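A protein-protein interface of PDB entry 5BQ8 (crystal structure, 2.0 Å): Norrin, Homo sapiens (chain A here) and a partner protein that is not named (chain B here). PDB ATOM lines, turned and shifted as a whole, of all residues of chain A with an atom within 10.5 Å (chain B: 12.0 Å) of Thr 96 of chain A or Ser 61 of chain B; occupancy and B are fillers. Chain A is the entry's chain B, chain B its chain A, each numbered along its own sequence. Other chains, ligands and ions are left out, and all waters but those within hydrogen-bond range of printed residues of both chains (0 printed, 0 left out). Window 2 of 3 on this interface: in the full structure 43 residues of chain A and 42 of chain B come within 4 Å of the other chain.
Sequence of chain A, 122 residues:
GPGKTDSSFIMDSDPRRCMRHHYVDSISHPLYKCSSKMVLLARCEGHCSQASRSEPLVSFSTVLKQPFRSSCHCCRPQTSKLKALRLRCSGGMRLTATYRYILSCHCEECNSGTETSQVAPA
The backbone carbonyl oxygen (O) of Ser 59 of chain B lies within hydrogen-bond range of the backbone NH (N) of Thr 98 of chain A (2.9 Å).
The backbone NH (N) of Leu 85 of chain A is in hydrogen-bond range of the backbone carbonyl oxygen (O) of Ala 97 of chain A, at 3.0 Å. O of MLY 83 of chain A lies within hydrogen-bond range of OG1 of Thr 98 of chain A (2.7 Å). The backbone NH of Leu 31 of chain A is in hydrogen-bond range of a ring nitrogen (ND1) of His 29 of chain A, 3.2 Å away. OG of Ser 59 of chain B sits at hydrogen-bond distance from N of MLY 65 of chain B (2.9 Å). N of Tyr 32 of chain A lies within hydrogen-bond range of ND1 of His 29 of chain A, 3.2 Å away. N of Leu 87 of chain A lies within hydrogen-bond range of O of Leu 95 of chain A, 2.9 Å away.
Val 58 of chain B touches Ile 27 of chain A. Ile 27 of chain A touches Phe 60 of chain B (CG2 to CE1, 3.6 Å). Ser 28 of chain A touches Phe 60 of chain B (O to CZ, 3.4 Å). His 29 of chain A touches Phe 60 of chain B. His 29 of chain A touches Ser 61 of chain B. Leu 31 of chain A touches Val 63 of chain B. Leu 87 of chain A touches Phe 60 of chain B (CD1 to CE1, 3.9 Å). Thr 96 of chain A touches Phe 60 of chain B. Ala 97 of chain A touches Ser 59 of chain B. Phe 60 of chain B touches Ala 97 of chain A.
Of the printed residues of chain B, Ile 27 of chain A touches Val 58 (3.9 Å) and Phe 60 (3.6 Å). Printed residues of chain B within 4 Å of Ser 28 of chain A: Phe 60. Leu 87 of chain A touches just one residue of chain B: Phe 60 (3.9 Å). Thr 96 of chain A touches two residues of chain B. Of chain B, only Val 58, Ser 59 and Phe 60 come within 4 Å of Ala 97 of chain A. Thr 98 of chain A touches just these residues of chain B: Val 58 (3.4 Å) and Ser 59 (2.9 Å). Printed residues of chain A within 4 Å of Val 58 of chain B: Ile 27, Ala 97 and Thr 98. Of the printed residues of chain A, Ser 59 of chain B touches Ala 97 (3.3 Å) and Thr 98 (2.9 Å). No residue of chain A comes within 4 Å of Thr 62 of chain B. Val 63 of chain B touches just one residue of chain A: Leu 31 (3.6 Å). The nearest residue of chain B that does not touch Thr 96 of chain A is Ser 59 of chain B (4.2 Å).
Hydrophobic or aromatic side chains of chain A that line the printed part of chain B: Ile 27, His 29, Pro 30, Leu 31, Leu 87 and Ala 97. Among the printed residues, 15 pairs touch across the chains. Among the printed residues, no Asp or Glu carboxylate lies within 4 Å of a Lys or Arg side-chain nitrogen of the other chain.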
ATOM      1  N   ILE A  27      -3.460  -3.519   7.475  1.00  0.00           N
ATOM      2  CA  ILE A  27      -2.710  -4.190   8.534  1.00  0.00           C
ATOM      3  C   ILE A  27      -3.226  -5.590   8.838  1.00  0.00           C
ATOM      4  O   ILE A  27      -4.418  -5.790   9.052  1.00  0.00           O
ATOM      5  CB  ILE A  27      -2.705  -3.358   9.823  1.00  0.00           C
ATOM      6  CG1 ILE A  27      -1.830  -2.127   9.615  1.00  0.00           C
ATOM      7  CG2 ILE A  27      -2.154  -4.169  10.995  1.00  0.00           C
ATOM      8  CD1 ILE A  27      -1.917  -1.115  10.717  1.00  0.00           C
ATOM      9  N   SER A  28      -2.305  -6.548   8.872  1.00  0.00           N
ATOM     10  CA  SER A  28      -2.624  -7.928   9.225  1.00  0.00           C
ATOM     11  C   SER A  28      -1.613  -8.473  10.223  1.00  0.00           C
ATOM     12  O   SER A  28      -0.423  -8.178  10.131  1.00  0.00           O
ATOM     13  CB  SER A  28      -2.613  -8.809   7.978  1.00  0.00           C
ATOM     14  OG  SER A  28      -1.289  -8.958   7.489  1.00  0.00           O
ATOM     15  N   HIS A  29      -2.082  -9.291  11.162  1.00  0.00           N
ATOM     16  CA  HIS A  29      -1.177  -9.891  12.133  1.00  0.00           C
ATOM     17  C   HIS A  29      -0.387 -11.000  11.433  1.00  0.00           C
ATOM     18  O   HIS A  29      -0.980 -11.884  10.814  1.00  0.00           O
ATOM     19  CB  HIS A  29      -1.950 -10.446  13.331  1.00  0.00           C
ATOM     20  CG  HIS A  29      -1.101 -10.657  14.543  1.00  0.00           C
ATOM     21  ND1 HIS A  29      -0.153 -11.650  14.622  1.00  0.00           N
ATOM     22  CD2 HIS A  29      -1.065 -10.002  15.728  1.00  0.00           C
ATOM     23  CE1 HIS A  29       0.442 -11.596  15.804  1.00  0.00           C
ATOM     24  NE2 HIS A  29      -0.096 -10.606  16.492  1.00  0.00           N
ATOM     25  N   PRO A  30       0.952 -10.970  11.534  1.00  0.00           N
ATOM     26  CA  PRO A  30       1.753 -11.956  10.791  1.00  0.00           C
ATOM     27  C   PRO A  30       1.745 -13.381  11.346  1.00  0.00           C
ATOM     28  O   PRO A  30       2.060 -14.319  10.612  1.00  0.00           O
ATOM     29  CB  PRO A  30       3.169 -11.377  10.877  1.00  0.00           C
ATOM     30  CG  PRO A  30       3.163 -10.561  12.123  1.00  0.00           C
ATOM     31  CD  PRO A  30       1.801  -9.951  12.176  1.00  0.00           C
ATOM     32  N   LEU A  31       1.374 -13.538  12.611  1.00  0.00           N
ATOM     33  CA  LEU A  31       1.438 -14.831  13.289  1.00  0.00           C
ATOM     34  C   LEU A  31       0.049 -15.385  13.625  1.00  0.00           C
ATOM     35  O   LEU A  31      -0.078 -16.538  14.049  1.00  0.00           O
ATOM     36  CB  LEU A  31       2.311 -14.716  14.550  1.00  0.00           C
ATOM     37  CG  LEU A  31       3.775 -14.336  14.260  1.00  0.00           C
ATOM     38  CD1 LEU A  31       4.579 -14.181  15.545  1.00  0.00           C
ATOM     39  CD2 LEU A  31       4.454 -15.343  13.330  1.00  0.00           C
ATOM     40  N   TYR A  32      -0.969 -14.528  13.540  1.00  0.00           N
ATOM     41  CA  TYR A  32      -2.338 -14.922  13.849  1.00  0.00           C
ATOM     42  C   TYR A  32      -3.329 -14.611  12.723  1.00  0.00           C
ATOM     43  O   TYR A  32      -3.211 -13.593  12.041  1.00  0.00           O
ATOM     44  CB  TYR A  32      -2.764 -14.242  15.140  1.00  0.00           C
ATOM     45  CG  TYR A  32      -3.719 -15.050  15.977  1.00  0.00           C
ATOM     46  CD1 TYR A  32      -3.268 -16.134  16.720  1.00  0.00           C
ATOM     47  CD2 TYR A  32      -5.061 -14.711  16.055  1.00  0.00           C
ATOM     48  CE1 TYR A  32      -4.135 -16.873  17.498  1.00  0.00           C
ATOM     49  CE2 TYR A  32      -5.933 -15.439  16.833  1.00  0.00           C
ATOM     50  CZ  TYR A  32      -5.465 -16.519  17.554  1.00  0.00           C
ATOM     51  OH  TYR A  32      -6.329 -17.249  18.333  1.00  0.00           O
ATOM     52  N   CYS A  34      -6.137 -12.971  11.347  1.00  0.00           N
ATOM     53  CA  CYS A  34      -6.970 -11.812  11.629  1.00  0.00           C
ATOM     54  C   CYS A  34      -7.499 -11.211  10.343  1.00  0.00           C
ATOM     55  O   CYS A  34      -6.899 -11.362   9.280  1.00  0.00           O
ATOM     56  CB  CYS A  34      -6.189 -10.761  12.418  1.00  0.00           C
ATOM     57  SG  CYS A  34      -5.564 -11.337  14.009  1.00  0.00           S
ATOM     58  N   LYS A  37      -7.256  -4.702   8.441  1.00  0.00           N
ATOM     59  CA  LYS A  37      -7.870  -3.428   8.794  1.00  0.00           C
ATOM     60  C   LYS A  37      -7.115  -2.302   8.102  1.00  0.00           C
ATOM     61  O   LYS A  37      -5.882  -2.294   8.070  1.00  0.00           O
ATOM     62  CB  LYS A  37      -7.855  -3.177  10.305  1.00  0.00           C
ATOM     63  CG  LYS A  37      -8.752  -2.010  10.718  1.00  0.00           C
ATOM     64  CD  LYS A  37      -9.135  -2.008  12.196  1.00  0.00           C
ATOM     65  CE  LYS A  37     -10.198  -3.020  12.574  1.00  0.00           C
ATOM     66  NZ  LYS A  37     -10.706  -2.719  13.948  1.00  0.00           N
ATOM     67  N   LEU A  82       2.110   7.823  19.514  1.00  0.00           N
ATOM     68  CA  LEU A  82       1.908   6.383  19.519  1.00  0.00           C
ATOM     69  C   LEU A  82       0.410   6.118  19.476  1.00  0.00           C
ATOM     70  O   LEU A  82      -0.344   6.682  20.266  1.00  0.00           O
ATOM     71  CB  LEU A  82       2.536   5.730  20.750  1.00  0.00           C
ATOM     72  CG  LEU A  82       2.403   4.206  20.792  1.00  0.00           C
ATOM     73  CD1 LEU A  82       3.180   3.563  19.647  1.00  0.00           C
ATOM     74  CD2 LEU A  82       2.866   3.658  22.129  1.00  0.00           C
ATOM     75  N   MLY A  83      -0.013   5.271  18.542  1.00  0.00           N
ATOM     76  CA  MLY A  83      -1.417   4.910  18.401  1.00  0.00           C
ATOM     77  CB  MLY A  83      -1.991   5.510  17.124  1.00  0.00           C
ATOM     78  CG  MLY A  83      -2.007   7.020  17.141  1.00  0.00           C
ATOM     79  CD  MLY A  83      -2.762   7.577  15.956  1.00  0.00           C
ATOM     80  CE  MLY A  83      -4.258   7.353  16.092  1.00  0.00           C
ATOM     81  NZ  MLY A  83      -5.035   8.504  15.549  1.00  0.00           N
ATOM     82  CH1 MLY A  83      -4.835   8.554  14.092  1.00  0.00           C
ATOM     83  CH2 MLY A  83      -6.453   8.203  15.774  1.00  0.00           C
ATOM     84  C   MLY A  83      -1.583   3.401  18.380  1.00  0.00           C
ATOM     85  O   MLY A  83      -0.614   2.664  18.214  1.00  0.00           O
ATOM     86  N   ALA A  84      -2.822   2.949  18.527  1.00  0.00           N
ATOM     87  CA  ALA A  84      -3.107   1.530  18.679  1.00  0.00           C
ATOM     88  C   ALA A  84      -4.499   1.195  18.168  1.00  0.00           C
ATOM     89  O   ALA A  84      -5.380   2.049  18.138  1.00  0.00           O
ATOM     90  CB  ALA A  84      -2.965   1.113  20.139  1.00  0.00           C
ATOM     91  N   LEU A  85      -4.682  -0.056  17.759  1.00  0.00           N
ATOM     92  CA  LEU A  85      -5.966  -0.521  17.260  1.00  0.00           C
ATOM     93  C   LEU A  85      -6.165  -1.995  17.579  1.00  0.00           C
ATOM     94  O   LEU A  85      -5.204  -2.761  17.717  1.00  0.00           O
ATOM     95  CB  LEU A  85      -6.103  -0.290  15.755  1.00  0.00           C
ATOM     96  CG  LEU A  85      -5.154  -0.984  14.777  1.00  0.00           C
ATOM     97  CD1 LEU A  85      -5.560  -2.430  14.503  1.00  0.00           C
ATOM     98  CD2 LEU A  85      -5.123  -0.208  13.478  1.00  0.00           C
ATOM     99  N   ARG A  86      -7.430  -2.361  17.736  1.00  0.00           N
ATOM    100  CA  ARG A  86      -7.830  -3.725  18.028  1.00  0.00           C
ATOM    101  C   ARG A  86      -8.162  -4.427  16.723  1.00  0.00           C
ATOM    102  O   ARG A  86      -9.004  -3.967  15.953  1.00  0.00           O
ATOM    103  CB  ARG A  86      -9.045  -3.714  18.949  1.00  0.00           C
ATOM    104  CG  ARG A  86      -8.765  -3.128  20.315  1.00  0.00           C
ATOM    105  CD  ARG A  86     -10.014  -3.100  21.174  1.00  0.00           C
ATOM    106  NE  ARG A  86     -10.948  -2.132  20.599  1.00  0.00           N
ATOM    107  CZ  ARG A  86     -12.206  -1.950  20.985  1.00  0.00           C
ATOM    108  NH1 ARG A  86     -12.950  -1.044  20.364  1.00  0.00           N
ATOM    109  NH2 ARG A  86     -12.718  -2.644  21.993  1.00  0.00           N
ATOM    110  N   LEU A  87      -7.502  -5.552  16.489  1.00  0.00           N
ATOM    111  CA  LEU A  87      -7.781  -6.383  15.332  1.00  0.00           C
ATOM    112  C   LEU A  87      -8.872  -7.366  15.698  1.00  0.00           C
ATOM    113  O   LEU A  87      -9.105  -7.624  16.879  1.00  0.00           O
ATOM    114  CB  LEU A  87      -6.516  -7.124  14.887  1.00  0.00           C
ATOM    115  CG  LEU A  87      -5.350  -6.271  14.393  1.00  0.00           C
ATOM    116  CD1 LEU A  87      -4.121  -7.124  14.154  1.00  0.00           C
ATOM    117  CD2 LEU A  87      -5.752  -5.620  13.087  1.00  0.00           C
ATOM    118  N   ARG A  88      -9.549  -7.896  14.687  1.00  0.00           N
ATOM    119  CA  ARG A  88     -10.553  -8.924  14.896  1.00  0.00           C
ATOM    120  C   ARG A  88      -9.990 -10.182  14.278  1.00  0.00           C
ATOM    121  O   ARG A  88      -9.663 -10.216  13.090  1.00  0.00           O
ATOM    122  CB  ARG A  88     -11.904  -8.550  14.281  1.00  0.00           C
ATOM    123  CG  ARG A  88     -12.469  -7.243  14.807  1.00  0.00           C
ATOM    124  CD  ARG A  88     -13.876  -6.989  14.301  1.00  0.00           C
ATOM    125  NE  ARG A  88     -14.493  -5.878  15.020  1.00  0.00           N
ATOM    126  CZ  ARG A  88     -15.193  -6.009  16.145  1.00  0.00           C
ATOM    127  NH1 ARG A  88     -15.365  -7.206  16.697  1.00  0.00           N
ATOM    128  NH2 ARG A  88     -15.716  -4.940  16.728  1.00  0.00           N
ATOM    129  N   CYS A  89      -9.881 -11.218  15.100  1.00  0.00           N
ATOM    130  CA  CYS A  89      -9.202 -12.433  14.706  1.00  0.00           C
ATOM    131  C   CYS A  89     -10.063 -13.647  14.996  1.00  0.00           C
ATOM    132  O   CYS A  89     -11.171 -13.525  15.519  1.00  0.00           O
ATOM    133  CB  CYS A  89      -7.865 -12.527  15.448  1.00  0.00           C
ATOM    134  SG  CYS A  89      -6.927 -10.974  15.471  1.00  0.00           S
ATOM    135  N   MET A  93     -11.245 -13.356  18.924  1.00  0.00           N
ATOM    136  CA  MET A  93     -10.047 -12.880  19.607  1.00  0.00           C
ATOM    137  C   MET A  93      -9.729 -11.474  19.136  1.00  0.00           C
ATOM    138  O   MET A  93      -9.863 -11.167  17.951  1.00  0.00           O
ATOM    139  CB  MET A  93      -8.857 -13.810  19.353  1.00  0.00           C
ATOM    140  CG  MET A  93      -8.962 -15.161  20.039  1.00  0.00           C
ATOM    141  SD  MET A  93      -8.892 -15.018  21.835  1.00  0.00           S
ATOM    142  CE  MET A  93      -8.912 -16.742  22.311  1.00  0.00           C
ATOM    143  N   ARG A  94      -9.328 -10.618  20.072  1.00  0.00           N
ATOM    144  CA  ARG A  94      -8.917  -9.263  19.735  1.00  0.00           C
ATOM    145  C   ARG A  94      -7.435  -9.075  20.053  1.00  0.00           C
ATOM    146  O   ARG A  94      -7.028  -9.153  21.213  1.00  0.00           O
ATOM    147  CB  ARG A  94      -9.754  -8.242  20.508  1.00  0.00           C
ATOM    148  CG  ARG A  94     -11.260  -8.494  20.467  1.00  0.00           C
ATOM    149  CD  ARG A  94     -11.860  -8.336  19.085  1.00  0.00           C
ATOM    150  NE  ARG A  94     -11.683  -6.995  18.542  1.00  0.00           N
ATOM    151  CZ  ARG A  94     -12.487  -5.966  18.794  1.00  0.00           C
ATOM    152  NH1 ARG A  94     -12.241  -4.787  18.242  1.00  0.00           N
ATOM    153  NH2 ARG A  94     -13.524  -6.105  19.610  1.00  0.00           N
ATOM    154  N   LEU A  95      -6.637  -8.822  19.018  1.00  0.00           N
ATOM    155  CA  LEU A  95      -5.192  -8.646  19.171  1.00  0.00           C
ATOM    156  C   LEU A  95      -4.772  -7.223  18.829  1.00  0.00           C
ATOM    157  O   LEU A  95      -5.207  -6.656  17.827  1.00  0.00           O
ATOM    158  CB  LEU A  95      -4.423  -9.647  18.311  1.00  0.00           C
ATOM    159  CG  LEU A  95      -4.779 -11.115  18.540  1.00  0.00           C
ATOM    160  CD1 LEU A  95      -3.896 -12.005  17.687  1.00  0.00           C
ATOM    161  CD2 LEU A  95      -4.679 -11.497  20.010  1.00  0.00           C
ATOM    162  N   THR A  96      -3.903  -6.666  19.664  1.00  0.00           N
ATOM    163  CA  THR A  96      -3.472  -5.285  19.528  1.00  0.00           C
ATOM    164  C   THR A  96      -2.354  -5.097  18.509  1.00  0.00           C
ATOM    165  O   THR A  96      -1.439  -5.914  18.406  1.00  0.00           O
ATOM    166  CB  THR A  96      -2.979  -4.739  20.883  1.00  0.00           C
ATOM    167  OG1 THR A  96      -4.022  -4.851  21.855  1.00  0.00           O
ATOM    168  CG2 THR A  96      -2.548  -3.284  20.769  1.00  0.00           C
ATOM    169  N   ALA A  97      -2.469  -4.018  17.741  1.00  0.00           N
ATOM    170  CA  ALA A  97      -1.421  -3.562  16.837  1.00  0.00           C
ATOM    171  C   ALA A  97      -1.114  -2.117  17.200  1.00  0.00           C
ATOM    172  O   ALA A  97      -2.028  -1.369  17.542  1.00  0.00           O
ATOM    173  CB  ALA A  97      -1.857  -3.679  15.394  1.00  0.00           C
ATOM    174  N   THR A  98       0.152  -1.713  17.124  1.00  0.00           N
ATOM    175  CA  THR A  98       0.523  -0.364  17.535  1.00  0.00           C
ATOM    176  C   THR A  98       1.509   0.230  16.534  1.00  0.00           C
ATOM    177  O   THR A  98       2.207  -0.498  15.830  1.00  0.00           O
ATOM    178  CB  THR A  98       1.140  -0.341  18.955  1.00  0.00           C
ATOM    179  OG1 THR A  98       1.005   0.968  19.520  1.00  0.00           O
ATOM    180  CG2 THR A  98       2.607  -0.776  18.948  1.00  0.00           C
ATOM    181  N   TYR A  99       1.536   1.554  16.452  1.00  0.00           N
ATOM    182  CA  TYR A  99       2.377   2.243  15.483  1.00  0.00           C
ATOM    183  C   TYR A  99       2.452   3.723  15.807  1.00  0.00           C
ATOM    184  O   TYR A  99       1.589   4.259  16.502  1.00  0.00           O
ATOM    185  CB  TYR A  99       1.823   2.061  14.071  1.00  0.00           C
ATOM    186  CG  TYR A  99       0.441   2.656  13.906  1.00  0.00           C
ATOM    187  CD1 TYR A  99       0.272   3.984  13.532  1.00  0.00           C
ATOM    188  CD2 TYR A  99      -0.694   1.893  14.134  1.00  0.00           C
ATOM    189  CE1 TYR A  99      -0.986   4.533  13.389  1.00  0.00           C
ATOM    190  CE2 TYR A  99      -1.958   2.434  13.992  1.00  0.00           C
ATOM    191  CZ  TYR A  99      -2.096   3.754  13.620  1.00  0.00           C
ATOM    192  OH  TYR A  99      -3.349   4.297  13.479  1.00  0.00           O
ATOM    193  N   LEU B  57       6.755   1.394  11.407  1.00  0.00           N
ATOM    194  CA  LEU B  57       6.614  -0.053  11.419  1.00  0.00           C
ATOM    195  C   LEU B  57       5.546  -0.402  12.446  1.00  0.00           C
ATOM    196  O   LEU B  57       5.469   0.227  13.503  1.00  0.00           O
ATOM    197  CB  LEU B  57       7.934  -0.741  11.766  1.00  0.00           C
ATOM    198  CG  LEU B  57       9.000  -0.792  10.672  1.00  0.00           C
ATOM    199  CD1 LEU B  57      10.329  -1.240  11.259  1.00  0.00           C
ATOM    200  CD2 LEU B  57       8.575  -1.723   9.547  1.00  0.00           C
ATOM    201  N   VAL B  58       4.718  -1.391  12.133  1.00  0.00           N
ATOM    202  CA  VAL B  58       3.652  -1.809  13.037  1.00  0.00           C
ATOM    203  C   VAL B  58       4.128  -2.943  13.941  1.00  0.00           C
ATOM    204  O   VAL B  58       4.714  -3.921  13.472  1.00  0.00           O
ATOM    205  CB  VAL B  58       2.399  -2.261  12.270  1.00  0.00           C
ATOM    206  CG1 VAL B  58       1.287  -2.676  13.242  1.00  0.00           C
ATOM    207  CG2 VAL B  58       1.911  -1.151  11.351  1.00  0.00           C
ATOM    208  N   SER B  59       3.890  -2.787  15.239  1.00  0.00           N
ATOM    209  CA  SER B  59       4.217  -3.826  16.205  1.00  0.00           C
ATOM    210  C   SER B  59       2.944  -4.546  16.616  1.00  0.00           C
ATOM    211  O   SER B  59       1.863  -3.952  16.617  1.00  0.00           O
ATOM    212  CB  SER B  59       4.903  -3.220  17.429  1.00  0.00           C
ATOM    213  OG  SER B  59       6.268  -2.957  17.163  1.00  0.00           O
ATOM    214  N   PHE B  60       3.074  -5.824  16.957  1.00  0.00           N
ATOM    215  CA  PHE B  60       1.948  -6.615  17.441  1.00  0.00           C
ATOM    216  C   PHE B  60       2.341  -7.346  18.711  1.00  0.00           C
ATOM    217  O   PHE B  60       3.507  -7.347  19.107  1.00  0.00           O
ATOM    218  CB  PHE B  60       1.507  -7.642  16.398  1.00  0.00           C
ATOM    219  CG  PHE B  60       1.179  -7.054  15.059  1.00  0.00           C
ATOM    220  CD1 PHE B  60      -0.097  -6.603  14.776  1.00  0.00           C
ATOM    221  CD2 PHE B  60       2.151  -6.966  14.076  1.00  0.00           C
ATOM    222  CE1 PHE B  60      -0.396  -6.067  13.539  1.00  0.00           C
ATOM    223  CE2 PHE B  60       1.859  -6.430  12.839  1.00  0.00           C
ATOM    224  CZ  PHE B  60       0.583  -5.981  12.569  1.00  0.00           C
ATOM    225  N   SER B  61       1.364  -7.978  19.341  1.00  0.00           N
ATOM    226  CA  SER B  61       1.612  -8.727  20.560  1.00  0.00           C
ATOM    227  C   SER B  61       2.684  -9.781  20.287  1.00  0.00           C
ATOM    228  O   SER B  61       2.545 -10.591  19.371  1.00  0.00           O
ATOM    229  CB  SER B  61       0.324  -9.365  21.059  1.00  0.00           C
ATOM    230  OG  SER B  61      -0.807  -8.720  20.493  1.00  0.00           O
ATOM    231  N   THR B  62       3.756  -9.737  21.075  1.00  0.00           N
ATOM    232  CA  THR B  62       4.911 -10.635  20.953  1.00  0.00           C
ATOM    233  C   THR B  62       5.746 -10.363  19.698  1.00  0.00           C
ATOM    234  O   THR B  62       6.705 -11.088  19.432  1.00  0.00           O
ATOM    235  CB  THR B  62       4.509 -12.133  20.930  1.00  0.00           C
ATOM    236  OG1 THR B  62       4.044 -12.505  19.626  1.00  0.00           O
ATOM    237  CG2 THR B  62       3.453 -12.448  21.984  1.00  0.00           C
ATOM    238  N   VAL B  63       5.372  -9.350  18.916  1.00  0.00           N
ATOM    239  CA  VAL B  63       6.157  -8.955  17.749  1.00  0.00           C
ATOM    240  C   VAL B  63       6.478  -7.466  17.812  1.00  0.00           C
ATOM    241  O   VAL B  63       5.765  -6.631  17.250  1.00  0.00           O
ATOM    242  CB  VAL B  63       5.443  -9.276  16.425  1.00  0.00           C
ATOM    243  CG1 VAL B  63       6.377  -9.021  15.247  1.00  0.00           C
ATOM    244  CG2 VAL B  63       4.972 -10.716  16.412  1.00  0.00           C
ATOM    245  N   LEU B  64       7.564  -7.149  18.504  1.00  0.00           N
ATOM    246  CA  LEU B  64       8.010  -5.774  18.682  1.00  0.00           C
ATOM    247  C   LEU B  64       9.028  -5.406  17.627  1.00  0.00           C
ATOM    248  O   LEU B  64       9.970  -6.156  17.366  1.00  0.00           O
ATOM    249  CB  LEU B  64       8.589  -5.598  20.079  1.00  0.00           C
ATOM    250  CG  LEU B  64       7.645  -5.089  21.167  1.00  0.00           C
ATOM    251  CD1 LEU B  64       6.237  -5.640  21.036  1.00  0.00           C
ATOM    252  CD2 LEU B  64       8.215  -5.531  22.498  1.00  0.00           C
ATOM    253  N   MLY B  65       8.817  -4.247  17.015  1.00  0.00           N
ATOM    254  CA  MLY B  65       9.716  -3.742  15.997  1.00  0.00           C
ATOM    255  CB  MLY B  65       9.046  -3.813  14.631  1.00  0.00           C
ATOM    256  CG  MLY B  65       8.899  -5.231  14.130  1.00  0.00           C
ATOM    257  CD  MLY B  65       7.863  -5.327  13.030  1.00  0.00           C
ATOM    258  CE  MLY B  65       8.480  -5.759  11.713  1.00  0.00           C
ATOM    259  NZ  MLY B  65       7.485  -6.446  10.843  1.00  0.00           N
ATOM    260  CH1 MLY B  65       6.449  -5.476  10.453  1.00  0.00           C
ATOM    261  CH2 MLY B  65       8.197  -6.837   9.622  1.00  0.00           C
ATOM    262  C   MLY B  65      10.090  -2.318  16.319  1.00  0.00           C
ATOM    263  O   MLY B  65       9.445  -1.667  17.146  1.00  0.00           O
